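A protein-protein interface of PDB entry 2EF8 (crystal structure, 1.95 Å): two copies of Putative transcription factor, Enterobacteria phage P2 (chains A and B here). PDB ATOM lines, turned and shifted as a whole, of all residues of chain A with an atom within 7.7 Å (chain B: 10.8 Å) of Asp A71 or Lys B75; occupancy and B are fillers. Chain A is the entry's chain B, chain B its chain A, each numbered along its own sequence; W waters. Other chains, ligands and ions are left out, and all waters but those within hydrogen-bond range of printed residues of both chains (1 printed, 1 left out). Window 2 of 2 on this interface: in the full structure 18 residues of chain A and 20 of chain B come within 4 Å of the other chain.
NZ of Lys B75 is in salt-bridge range of OD2 of Asp A71 (3.1 Å).
OG1 of Thr B77 is in hydrogen-bond range of O of Leu B73 (2.7 Å). The backbone carbonyl oxygen of Thr B77 is in hydrogen-bond range of the side-chain hydroxyl of Ser B80 (2.5 Å). OG1 of Thr A77 sits at hydrogen-bond distance from O of Leu A73.
Among the printed residues, pairs that only touch across the chains: Phe A56 with Leu B55 (3.5 Å), Phe A56 with Thr B77 (3.6 Å), Phe A56 with Tyr B78 (3.7 Å), Phe A56 with Ile B81 (3.6 Å), Met A70 with Tyr B78 (3.7 Å) and Thr A77 with Phe B56 (3.5 Å).
Asp A71 touches just one residue of chain B: Lys B75 (3.1 Å). Lys B75 touches one residue of chain A. No residue of chain B comes within 4 Å of Pro A69. Of chain B, only Tyr B78 (3.7 Å) comes within 4 Å of Met A70. Ile A72 touches none of the printed residues of chain B. No residue of chain B comes within 4 Å of Lys A75. Of the printed residues of chain B, Phe A56 touches Leu B55, Thr B77, Tyr B78 and Ile B81. Of the printed residues of chain A, Thr B77 touches Phe A56 (3.6 Å). The nearest residue of chain A that does not touch Lys B75 is Leu A74 (4.1 Å). The nearest printed residue of chain B that does not touch Thr A77 is Leu B74 (6.7 Å).
Of the 12 printed residues of chain A, 4 touch a printed residue of chain B. Hydrophobic or aromatic side chains of chain A within 4 Å of the printed part of chain B: Phe A56 and Met A70. Along chain A the printed residues that touch a printed residue of chain B span positions 56 to 77. Of the 24 printed residues of chain B, 6 touch a printed residue of chain A. Printed residues of chain B that touch a printed residue of chain A: Leu B55, Phe B56, Lys B75, Thr B77, Tyr B78 and Ile B81.
Phe A56 touches Thr B77, and with the chains exchanged Thr A77 touches Phe B56. Asp A71 touches Lys B75, but with the chains exchanged Lys A75 does not touch Asp B71 (5.6 Å). 12 positions are printed for both chains. Of the 7 pairs that touch across the chains among the printed residues, 2 have their exchanged pair printed and touching as well.
Water W1 bridges O of Asp B71 (2.8 Å) and OD2 of Asp A71 (2.8 Å).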
ATOM      1  N   PHE A  56       7.275 -26.221  -0.984  1.00  0.00           N
ATOM      2  CA  PHE A  56       7.169 -27.602  -0.497  1.00  0.00           C
ATOM      3  C   PHE A  56       7.898 -28.616  -1.384  1.00  0.00           C
ATOM      4  O   PHE A  56       8.600 -29.515  -0.882  1.00  0.00           O
ATOM      5  CB  PHE A  56       5.701 -28.027  -0.364  1.00  0.00           C
ATOM      6  CG  PHE A  56       4.988 -27.382   0.777  1.00  0.00           C
ATOM      7  CD1 PHE A  56       3.913 -26.531   0.544  1.00  0.00           C
ATOM      8  CD2 PHE A  56       5.372 -27.640   2.092  1.00  0.00           C
ATOM      9  CE1 PHE A  56       3.215 -25.943   1.592  1.00  0.00           C
ATOM     10  CE2 PHE A  56       4.681 -27.056   3.167  1.00  0.00           C
ATOM     11  CZ  PHE A  56       3.597 -26.205   2.921  1.00  0.00           C
ATOM     12  N   ALA A  63      14.980 -33.030   1.115  1.00  0.00           N
ATOM     13  CA  ALA A  63      14.855 -34.020   2.188  1.00  0.00           C
ATOM     14  C   ALA A  63      15.255 -35.397   1.671  1.00  0.00           C
ATOM     15  O   ALA A  63      16.008 -36.142   2.325  1.00  0.00           O
ATOM     16  CB  ALA A  63      13.396 -34.043   2.741  1.00  0.00           C
ATOM     17  N   LEU A  68      16.765 -36.697   5.152  1.00  0.00           N
ATOM     18  CA  LEU A  68      16.207 -36.032   6.327  1.00  0.00           C
ATOM     19  C   LEU A  68      14.677 -36.008   6.334  1.00  0.00           C
ATOM     20  O   LEU A  68      14.030 -35.956   5.284  1.00  0.00           O
ATOM     21  CB  LEU A  68      16.699 -34.584   6.403  1.00  0.00           C
ATOM     22  CG  LEU A  68      18.085 -34.251   6.954  1.00  0.00           C
ATOM     23  CD1 LEU A  68      18.361 -32.770   6.751  1.00  0.00           C
ATOM     24  CD2 LEU A  68      18.151 -34.611   8.432  1.00  0.00           C
ATOM     25  N   PRO A  69      14.080 -36.053   7.529  1.00  0.00           N
ATOM     26  CA  PRO A  69      12.616 -36.019   7.648  1.00  0.00           C
ATOM     27  C   PRO A  69      12.159 -34.637   7.162  1.00  0.00           C
ATOM     28  O   PRO A  69      12.895 -33.655   7.305  1.00  0.00           O
ATOM     29  CB  PRO A  69      12.378 -36.153   9.156  1.00  0.00           C
ATOM     30  CG  PRO A  69      13.642 -36.813   9.676  1.00  0.00           C
ATOM     31  CD  PRO A  69      14.731 -36.202   8.846  1.00  0.00           C
ATOM     32  N   MET A  70      10.955 -34.550   6.609  1.00  0.00           N
ATOM     33  CA  MET A  70      10.449 -33.259   6.155  1.00  0.00           C
ATOM     34  C   MET A  70      10.260 -32.325   7.352  1.00  0.00           C
ATOM     35  O   MET A  70      10.442 -31.117   7.219  1.00  0.00           O
ATOM     36  CB  MET A  70       9.118 -33.415   5.407  1.00  0.00           C
ATOM     37  CG  MET A  70       9.276 -33.582   3.885  1.00  0.00           C
ATOM     38  SD  MET A  70       9.964 -32.111   3.034  1.00  0.00           S
ATOM     39  CE  MET A  70       8.574 -30.970   3.107  1.00  0.00           C
ATOM     40  N   ASP A  71       9.876 -32.880   8.502  1.00  0.00           N
ATOM     41  CA  ASP A  71       9.688 -32.081   9.724  1.00  0.00           C
ATOM     42  C   ASP A  71      10.920 -31.215  10.024  1.00  0.00           C
ATOM     43  O   ASP A  71      10.799 -30.080  10.504  1.00  0.00           O
ATOM     44  CB  ASP A  71       9.443 -32.987  10.941  1.00  0.00           C
ATOM     45  CG  ASP A  71       8.026 -33.556  10.991  1.00  0.00           C
ATOM     46  OD1 ASP A  71       7.801 -34.497  11.786  1.00  0.00           O
ATOM     47  OD2 ASP A  71       7.138 -33.058  10.259  1.00  0.00           O
ATOM     48  N   ILE A  72      12.101 -31.769   9.768  1.00  0.00           N
ATOM     49  CA  ILE A  72      13.356 -31.070  10.028  1.00  0.00           C
ATOM     50  C   ILE A  72      13.563 -29.910   9.065  1.00  0.00           C
ATOM     51  O   ILE A  72      13.937 -28.816   9.482  1.00  0.00           O
ATOM     52  CB  ILE A  72      14.590 -32.040   9.941  1.00  0.00           C
ATOM     53  CG1 ILE A  72      14.707 -32.854  11.238  1.00  0.00           C
ATOM     54  CG2 ILE A  72      15.883 -31.258   9.724  1.00  0.00           C
ATOM     55  CD1 ILE A  72      15.178 -32.042  12.446  1.00  0.00           C
ATOM     56  N   LEU A  73      13.317 -30.140   7.780  1.00  0.00           N
ATOM     57  CA  LEU A  73      13.506 -29.067   6.810  1.00  0.00           C
ATOM     58  C   LEU A  73      12.437 -27.995   6.963  1.00  0.00           C
ATOM     59  O   LEU A  73      12.702 -26.814   6.759  1.00  0.00           O
ATOM     60  CB  LEU A  73      13.510 -29.633   5.391  1.00  0.00           C
ATOM     61  CG  LEU A  73      14.793 -30.430   5.084  1.00  0.00           C
ATOM     62  CD1 LEU A  73      14.675 -31.069   3.715  1.00  0.00           C
ATOM     63  CD2 LEU A  73      16.014 -29.493   5.131  1.00  0.00           C
ATOM     64  N   LEU A  74      11.227 -28.405   7.328  1.00  0.00           N
ATOM     65  CA  LEU A  74      10.155 -27.439   7.513  1.00  0.00           C
ATOM     66  C   LEU A  74      10.516 -26.514   8.671  1.00  0.00           C
ATOM     67  O   LEU A  74      10.348 -25.291   8.593  1.00  0.00           O
ATOM     68  CB  LEU A  74       8.838 -28.167   7.801  1.00  0.00           C
ATOM     69  CG  LEU A  74       8.241 -28.871   6.574  1.00  0.00           C
ATOM     70  CD1 LEU A  74       7.123 -29.821   6.998  1.00  0.00           C
ATOM     71  CD2 LEU A  74       7.732 -27.802   5.593  1.00  0.00           C
ATOM     72  N   LYS A  75      11.031 -27.116   9.735  1.00  0.00           N
ATOM     73  CA  LYS A  75      11.434 -26.388  10.931  1.00  0.00           C
ATOM     74  C   LYS A  75      12.593 -25.433  10.624  1.00  0.00           C
ATOM     75  O   LYS A  75      12.587 -24.283  11.060  1.00  0.00           O
ATOM     76  CB  LYS A  75      11.832 -27.389  12.026  1.00  0.00           C
ATOM     77  CG  LYS A  75      12.077 -26.763  13.382  1.00  0.00           C
ATOM     78  CD  LYS A  75      11.322 -27.521  14.486  1.00  0.00           C
ATOM     79  CE  LYS A  75      12.065 -28.771  14.986  1.00  0.00           C
ATOM     80  NZ  LYS A  75      12.263 -29.846  13.956  1.00  0.00           N
ATOM     81  N   ASP A  76      13.593 -25.921   9.891  1.00  0.00           N
ATOM     82  CA  ASP A  76      14.750 -25.101   9.511  1.00  0.00           C
ATOM     83  C   ASP A  76      14.263 -23.850   8.774  1.00  0.00           C
ATOM     84  O   ASP A  76      14.665 -22.717   9.065  1.00  0.00           O
ATOM     85  CB  ASP A  76      15.658 -25.861   8.535  1.00  0.00           C
ATOM     86  CG  ASP A  76      16.411 -27.011   9.173  1.00  0.00           C
ATOM     87  OD1 ASP A  76      16.894 -27.893   8.407  1.00  0.00           O
ATOM     88  OD2 ASP A  76      16.542 -27.032  10.411  1.00  0.00           O
ATOM     89  N   THR A  77      13.397 -24.074   7.789  1.00  0.00           N
ATOM     90  CA  THR A  77      12.908 -22.979   6.973  1.00  0.00           C
ATOM     91  C   THR A  77      12.013 -22.021   7.755  1.00  0.00           C
ATOM     92  O   THR A  77      12.185 -20.814   7.653  1.00  0.00           O
ATOM     93  CB  THR A  77      12.111 -23.536   5.758  1.00  0.00           C
ATOM     94  OG1 THR A  77      12.848 -24.607   5.153  1.00  0.00           O
ATOM     95  CG2 THR A  77      11.888 -22.460   4.717  1.00  0.00           C
ATOM     96  N   LEU B  11      -3.803 -26.204  -3.059  1.00  0.00           N
ATOM     97  CA  LEU B  11      -3.118 -25.690  -1.881  1.00  0.00           C
ATOM     98  C   LEU B  11      -3.715 -24.335  -1.464  1.00  0.00           C
ATOM     99  O   LEU B  11      -4.003 -24.097  -0.284  1.00  0.00           O
ATOM    100  CB  LEU B  11      -1.623 -25.539  -2.193  1.00  0.00           C
ATOM    101  CG  LEU B  11      -0.767 -24.840  -1.129  1.00  0.00           C
ATOM    102  CD1 LEU B  11      -0.892 -25.536   0.232  1.00  0.00           C
ATOM    103  CD2 LEU B  11       0.705 -24.845  -1.610  1.00  0.00           C
ATOM    104  N   LEU B  14      -7.074 -24.722   0.248  1.00  0.00           N
ATOM    105  CA  LEU B  14      -6.937 -25.182   1.629  1.00  0.00           C
ATOM    106  C   LEU B  14      -6.530 -24.026   2.548  1.00  0.00           C
ATOM    107  O   LEU B  14      -7.038 -23.894   3.659  1.00  0.00           O
ATOM    108  CB  LEU B  14      -5.883 -26.302   1.727  1.00  0.00           C
ATOM    109  CG  LEU B  14      -5.331 -26.533   3.145  1.00  0.00           C
ATOM    110  CD1 LEU B  14      -6.454 -26.882   4.086  1.00  0.00           C
ATOM    111  CD2 LEU B  14      -4.301 -27.650   3.142  1.00  0.00           C
ATOM    112  N   LEU B  15      -5.596 -23.204   2.082  1.00  0.00           N
ATOM    113  CA  LEU B  15      -5.121 -22.065   2.865  1.00  0.00           C
ATOM    114  C   LEU B  15      -6.250 -21.043   3.046  1.00  0.00           C
ATOM    115  O   LEU B  15      -6.356 -20.398   4.083  1.00  0.00           O
ATOM    116  CB  LEU B  15      -3.912 -21.426   2.158  1.00  0.00           C
ATOM    117  CG  LEU B  15      -2.662 -22.307   2.009  1.00  0.00           C
ATOM    118  CD1 LEU B  15      -1.557 -21.519   1.322  1.00  0.00           C
ATOM    119  CD2 LEU B  15      -2.183 -22.786   3.399  1.00  0.00           C
ATOM    120  N   LEU B  18      -8.276 -22.289   5.717  1.00  0.00           N
ATOM    121  CA  LEU B  18      -7.630 -22.080   7.011  1.00  0.00           C
ATOM    122  C   LEU B  18      -7.884 -20.664   7.524  1.00  0.00           C
ATOM    123  O   LEU B  18      -8.201 -20.460   8.699  1.00  0.00           O
ATOM    124  CB  LEU B  18      -6.111 -22.340   6.903  1.00  0.00           C
ATOM    125  CG  LEU B  18      -5.686 -23.801   6.708  1.00  0.00           C
ATOM    126  CD1 LEU B  18      -4.163 -23.907   6.732  1.00  0.00           C
ATOM    127  CD2 LEU B  18      -6.281 -24.665   7.807  1.00  0.00           C
ATOM    128  N   LEU B  55       3.379 -17.808   2.443  1.00  0.00           N
ATOM    129  CA  LEU B  55       2.849 -19.086   2.916  1.00  0.00           C
ATOM    130  C   LEU B  55       3.139 -19.234   4.413  1.00  0.00           C
ATOM    131  O   LEU B  55       2.244 -19.564   5.204  1.00  0.00           O
ATOM    132  CB  LEU B  55       3.490 -20.250   2.152  1.00  0.00           C
ATOM    133  CG  LEU B  55       3.448 -21.636   2.819  1.00  0.00           C
ATOM    134  CD1 LEU B  55       2.044 -22.125   2.938  1.00  0.00           C
ATOM    135  CD2 LEU B  55       4.229 -22.599   1.998  1.00  0.00           C
ATOM    136  N   PHE B  56       4.386 -18.997   4.818  1.00  0.00           N
ATOM    137  CA  PHE B  56       4.714 -19.134   6.239  1.00  0.00           C
ATOM    138  C   PHE B  56       3.993 -18.093   7.085  1.00  0.00           C
ATOM    139  O   PHE B  56       3.533 -18.383   8.194  1.00  0.00           O
ATOM    140  CB  PHE B  56       6.238 -19.024   6.474  1.00  0.00           C
ATOM    141  CG  PHE B  56       7.001 -20.239   6.036  1.00  0.00           C
ATOM    142  CD1 PHE B  56       7.691 -20.252   4.829  1.00  0.00           C
ATOM    143  CD2 PHE B  56       7.021 -21.382   6.837  1.00  0.00           C
ATOM    144  CE1 PHE B  56       8.399 -21.390   4.416  1.00  0.00           C
ATOM    145  CE2 PHE B  56       7.722 -22.523   6.441  1.00  0.00           C
ATOM    146  CZ  PHE B  56       8.415 -22.524   5.218  1.00  0.00           C
ATOM    147  N   LEU B  59       0.338 -19.221   7.625  1.00  0.00           N
ATOM    148  CA  LEU B  59       0.222 -20.325   8.571  1.00  0.00           C
ATOM    149  C   LEU B  59       0.521 -19.867   9.998  1.00  0.00           C
ATOM    150  O   LEU B  59      -0.101 -20.341  10.955  1.00  0.00           O
ATOM    151  CB  LEU B  59       1.164 -21.464   8.182  1.00  0.00           C
ATOM    152  CG  LEU B  59       0.858 -22.153   6.855  1.00  0.00           C
ATOM    153  CD1 LEU B  59       1.898 -23.249   6.656  1.00  0.00           C
ATOM    154  CD2 LEU B  59      -0.565 -22.730   6.835  1.00  0.00           C
ATOM    155  N   ALA B  63      -2.111 -20.301  12.863  1.00  0.00           N
ATOM    156  CA  ALA B  63      -1.704 -21.115  14.007  1.00  0.00           C
ATOM    157  C   ALA B  63      -1.976 -20.407  15.324  1.00  0.00           C
ATOM    158  O   ALA B  63      -2.435 -21.025  16.291  1.00  0.00           O
ATOM    159  CB  ALA B  63      -0.210 -21.467  13.904  1.00  0.00           C
ATOM    160  N   LEU B  68      -2.984 -23.676  17.345  1.00  0.00           N
ATOM    161  CA  LEU B  68      -2.379 -24.898  16.818  1.00  0.00           C
ATOM    162  C   LEU B  68      -0.860 -24.759  16.716  1.00  0.00           C
ATOM    163  O   LEU B  68      -0.352 -23.685  16.439  1.00  0.00           O
ATOM    164  CB  LEU B  68      -2.937 -25.211  15.426  1.00  0.00           C
ATOM    165  CG  LEU B  68      -4.460 -25.303  15.262  1.00  0.00           C
ATOM    166  CD1 LEU B  68      -4.798 -25.549  13.808  1.00  0.00           C
ATOM    167  CD2 LEU B  68      -5.009 -26.437  16.128  1.00  0.00           C
ATOM    168  N   PRO B  69      -0.118 -25.845  16.969  1.00  0.00           N
ATOM    169  CA  PRO B  69       1.343 -25.767  16.867  1.00  0.00           C
ATOM    170  C   PRO B  69       1.765 -25.680  15.386  1.00  0.00           C
ATOM    171  O   PRO B  69       1.139 -26.303  14.520  1.00  0.00           O
ATOM    172  CB  PRO B  69       1.802 -27.061  17.545  1.00  0.00           C
ATOM    173  CG  PRO B  69       0.646 -27.990  17.339  1.00  0.00           C
ATOM    174  CD  PRO B  69      -0.533 -27.107  17.606  1.00  0.00           C
ATOM    175  N   MET B  70       2.796 -24.882  15.099  1.00  0.00           N
ATOM    176  CA  MET B  70       3.290 -24.713  13.732  1.00  0.00           C
ATOM    177  C   MET B  70       3.779 -25.999  13.093  1.00  0.00           C
ATOM    178  O   MET B  70       3.512 -26.249  11.922  1.00  0.00           O
ATOM    179  CB  MET B  70       4.430 -23.681  13.674  1.00  0.00           C
ATOM    180  CG  MET B  70       3.973 -22.241  13.462  1.00  0.00           C
ATOM    181  SD  MET B  70       3.069 -21.986  11.909  1.00  0.00           S
ATOM    182  CE  MET B  70       4.341 -22.146  10.729  1.00  0.00           C
ATOM    183  N   ASP B  71       4.504 -26.824  13.844  1.00  0.00           N
ATOM    184  CA  ASP B  71       5.008 -28.047  13.244  1.00  0.00           C
ATOM    185  C   ASP B  71       3.889 -28.932  12.696  1.00  0.00           C
ATOM    186  O   ASP B  71       4.034 -29.551  11.638  1.00  0.00           O
ATOM    187  CB  ASP B  71       5.899 -28.815  14.239  1.00  0.00           C
ATOM    188  CG  ASP B  71       5.123 -29.449  15.373  1.00  0.00           C
ATOM    189  OD1 ASP B  71       4.333 -28.749  16.043  1.00  0.00           O
ATOM    190  OD2 ASP B  71       5.321 -30.661  15.599  1.00  0.00           O
ATOM    191  N   ILE B  72       2.758 -28.984  13.390  1.00  0.00           N
ATOM    192  CA  ILE B  72       1.655 -29.800  12.904  1.00  0.00           C
ATOM    193  C   ILE B  72       1.005 -29.130  11.703  1.00  0.00           C
ATOM    194  O   ILE B  72       0.692 -29.790  10.724  1.00  0.00           O
ATOM    195  CB  ILE B  72       0.568 -30.035  13.991  1.00  0.00           C
ATOM    196  CG1 ILE B  72       1.209 -30.579  15.271  1.00  0.00           C
ATOM    197  CG2 ILE B  72      -0.485 -30.997  13.456  1.00  0.00           C
ATOM    198  CD1 ILE B  72       2.113 -31.786  15.074  1.00  0.00           C
ATOM    199  N   LEU B  73       0.805 -27.819  11.777  1.00  0.00           N
ATOM    200  CA  LEU B  73       0.191 -27.080  10.675  1.00  0.00           C
ATOM    201  C   LEU B  73       1.027 -27.237   9.407  1.00  0.00           C
ATOM    202  O   LEU B  73       0.507 -27.500   8.325  1.00  0.00           O
ATOM    203  CB  LEU B  73       0.114 -25.585  10.998  1.00  0.00           C
ATOM    204  CG  LEU B  73      -1.238 -24.876  10.995  1.00  0.00           C
ATOM    205  CD1 LEU B  73      -1.003 -23.375  10.896  1.00  0.00           C
ATOM    206  CD2 LEU B  73      -2.093 -25.362   9.833  1.00  0.00           C
ATOM    207  N   LEU B  74       2.330 -27.044   9.550  1.00  0.00           N
ATOM    208  CA  LEU B  74       3.241 -27.164   8.423  1.00  0.00           C
ATOM    209  C   LEU B  74       3.229 -28.559   7.824  1.00  0.00           C
ATOM    210  O   LEU B  74       3.131 -28.729   6.613  1.00  0.00           O
ATOM    211  CB  LEU B  74       4.672 -26.822   8.866  1.00  0.00           C
ATOM    212  CG  LEU B  74       5.050 -25.351   8.965  1.00  0.00           C
ATOM    213  CD1 LEU B  74       6.414 -25.205   9.618  1.00  0.00           C
ATOM    214  CD2 LEU B  74       5.076 -24.746   7.562  1.00  0.00           C
ATOM    215  N   LYS B  75       3.353 -29.566   8.674  1.00  0.00           N
ATOM    216  CA  LYS B  75       3.375 -30.935   8.175  1.00  0.00           C
ATOM    217  C   LYS B  75       2.077 -31.295   7.471  1.00  0.00           C
ATOM    218  O   LYS B  75       2.089 -31.870   6.373  1.00  0.00           O
ATOM    219  CB  LYS B  75       3.629 -31.917   9.317  1.00  0.00           C
ATOM    220  CG  LYS B  75       3.878 -33.333   8.820  1.00  0.00           C
ATOM    221  CD  LYS B  75       5.049 -33.343   7.818  1.00  0.00           C
ATOM    222  CE  LYS B  75       5.489 -34.753   7.472  1.00  0.00           C
ATOM    223  NZ  LYS B  75       5.935 -35.442   8.708  1.00  0.00           N
ATOM    224  N   ASP B  76       0.954 -30.962   8.105  1.00  0.00           N
ATOM    225  CA  ASP B  76      -0.344 -31.258   7.516  1.00  0.00           C
ATOM    226  C   ASP B  76      -0.531 -30.565   6.169  1.00  0.00           C
ATOM    227  O   ASP B  76      -1.048 -31.163   5.221  1.00  0.00           O
ATOM    228  CB  ASP B  76      -1.468 -30.831   8.463  1.00  0.00           C
ATOM    229  CG  ASP B  76      -1.753 -31.866   9.531  1.00  0.00           C
ATOM    230  OD1 ASP B  76      -0.979 -32.854   9.630  1.00  0.00           O
ATOM    231  OD2 ASP B  76      -2.742 -31.682  10.268  1.00  0.00           O
ATOM    232  N   THR B  77      -0.137 -29.295   6.099  1.00  0.00           N
ATOM    233  CA  THR B  77      -0.261 -28.533   4.861  1.00  0.00           C
ATOM    234  C   THR B  77       0.574 -29.222   3.794  1.00  0.00           C
ATOM    235  O   THR B  77       0.120 -29.453   2.676  1.00  0.00           O
ATOM    236  CB  THR B  77       0.214 -27.072   5.044  1.00  0.00           C
ATOM    237  OG1 THR B  77      -0.587 -26.420   6.052  1.00  0.00           O
ATOM    238  CG2 THR B  77       0.072 -26.315   3.737  1.00  0.00           C
ATOM    239  N   TYR B  78       1.808 -29.558   4.137  1.00  0.00           N
ATOM    240  CA  TYR B  78       2.659 -30.279   3.196  1.00  0.00           C
ATOM    241  C   TYR B  78       1.993 -31.583   2.748  1.00  0.00           C
ATOM    242  O   TYR B  78       1.922 -31.881   1.540  1.00  0.00           O
ATOM    243  CB  TYR B  78       4.000 -30.637   3.842  1.00  0.00           C
ATOM    244  CG  TYR B  78       4.777 -31.637   3.020  1.00  0.00           C
ATOM    245  CD1 TYR B  78       5.195 -31.321   1.727  1.00  0.00           C
ATOM    246  CD2 TYR B  78       5.045 -32.912   3.507  1.00  0.00           C
ATOM    247  CE1 TYR B  78       5.850 -32.252   0.932  1.00  0.00           C
ATOM    248  CE2 TYR B  78       5.707 -33.857   2.723  1.00  0.00           C
ATOM    249  CZ  TYR B  78       6.102 -33.517   1.434  1.00  0.00           C
ATOM    250  OH  TYR B  78       6.732 -34.443   0.641  1.00  0.00           O
ATOM    251  N   GLU B  79       1.507 -32.365   3.709  1.00  0.00           N
ATOM    252  CA  GLU B  79       0.901 -33.654   3.362  1.00  0.00           C
ATOM    253  C   GLU B  79      -0.397 -33.562   2.566  1.00  0.00           C
ATOM    254  O   GLU B  79      -0.830 -34.550   1.961  1.00  0.00           O
ATOM    255  CB  GLU B  79       0.653 -34.488   4.625  1.00  0.00           C
ATOM    256  CG  GLU B  79       1.918 -34.975   5.355  1.00  0.00           C
ATOM    257  CD  GLU B  79       2.826 -35.839   4.486  1.00  0.00           C
ATOM    258  OE1 GLU B  79       2.374 -36.317   3.423  1.00  0.00           O
ATOM    259  OE2 GLU B  79       3.997 -36.055   4.873  1.00  0.00           O
ATOM    260  N   SER B  80      -1.017 -32.386   2.557  1.00  0.00           N
ATOM    261  CA  SER B  80      -2.278 -32.204   1.831  1.00  0.00           C
ATOM    262  C   SER B  80      -2.034 -32.234   0.332  1.00  0.00           C
ATOM    263  O   SER B  80      -2.943 -32.490  -0.461  1.00  0.00           O
ATOM    264  CB  SER B  80      -2.926 -30.864   2.206  1.00  0.00           C
ATOM    265  OG  SER B  80      -2.197 -29.765   1.669  1.00  0.00           O
ATOM    266  N   ILE B  81      -0.801 -31.964  -0.059  1.00  0.00           N
ATOM    267  CA  ILE B  81      -0.470 -31.954  -1.466  1.00  0.00           C
ATOM    268  C   ILE B  81      -0.377 -33.388  -1.991  1.00  0.00           C
ATOM    269  O   ILE B  81       0.444 -34.178  -1.527  1.00  0.00           O
ATOM    270  CB  ILE B  81       0.860 -31.223  -1.703  1.00  0.00           C
ATOM    271  CG1 ILE B  81       0.770 -29.795  -1.150  1.00  0.00           C
ATOM    272  CG2 ILE B  81       1.177 -31.190  -3.193  1.00  0.00           C
ATOM    273  CD1 ILE B  81       2.055 -29.038  -1.245  1.00  0.00           C
ATOM    274  N   SER B  82      -1.238 -33.726  -2.944  1.00  0.00           N
ATOM    275  CA  SER B  82      -1.227 -35.071  -3.520  1.00  0.00           C
ATOM    276  C   SER B  82       0.113 -35.300  -4.188  1.00  0.00           C
ATOM    277  O   SER B  82       0.596 -34.436  -4.919  1.00  0.00           O
ATOM    278  CB  SER B  82      -2.337 -35.221  -4.563  1.00  0.00           C
ATOM    279  OG  SER B  82      -3.614 -35.034  -3.982  1.00  0.00           O
ATOM    280  N   LYS B  83       0.723 -36.453  -3.932  1.00  0.00           N
ATOM    281  CA  LYS B  83       2.009 -36.771  -4.545  1.00  0.00           C
ATOM    282  C   LYS B  83       1.748 -37.520  -5.846  1.00  0.00           C
ATOM    283  O   LYS B  83       2.656 -37.716  -6.657  1.00  0.00           O
ATOM    284  CB  LYS B  83       2.862 -37.629  -3.609  1.00  0.00           C
ATOM    285  CG  LYS B  83       3.325 -36.916  -2.347  1.00  0.00           C
ATOM    286  CD  LYS B  83       4.277 -37.809  -1.557  1.00  0.00           C
ATOM    287  CE  LYS B  83       4.760 -37.153  -0.277  1.00  0.00           C
ATOM    288  NZ  LYS B  83       5.692 -38.050   0.471  1.00  0.00           N
HETATM  289  O   HOH W   1       6.488 -30.322  10.627  1.00  0.00           O
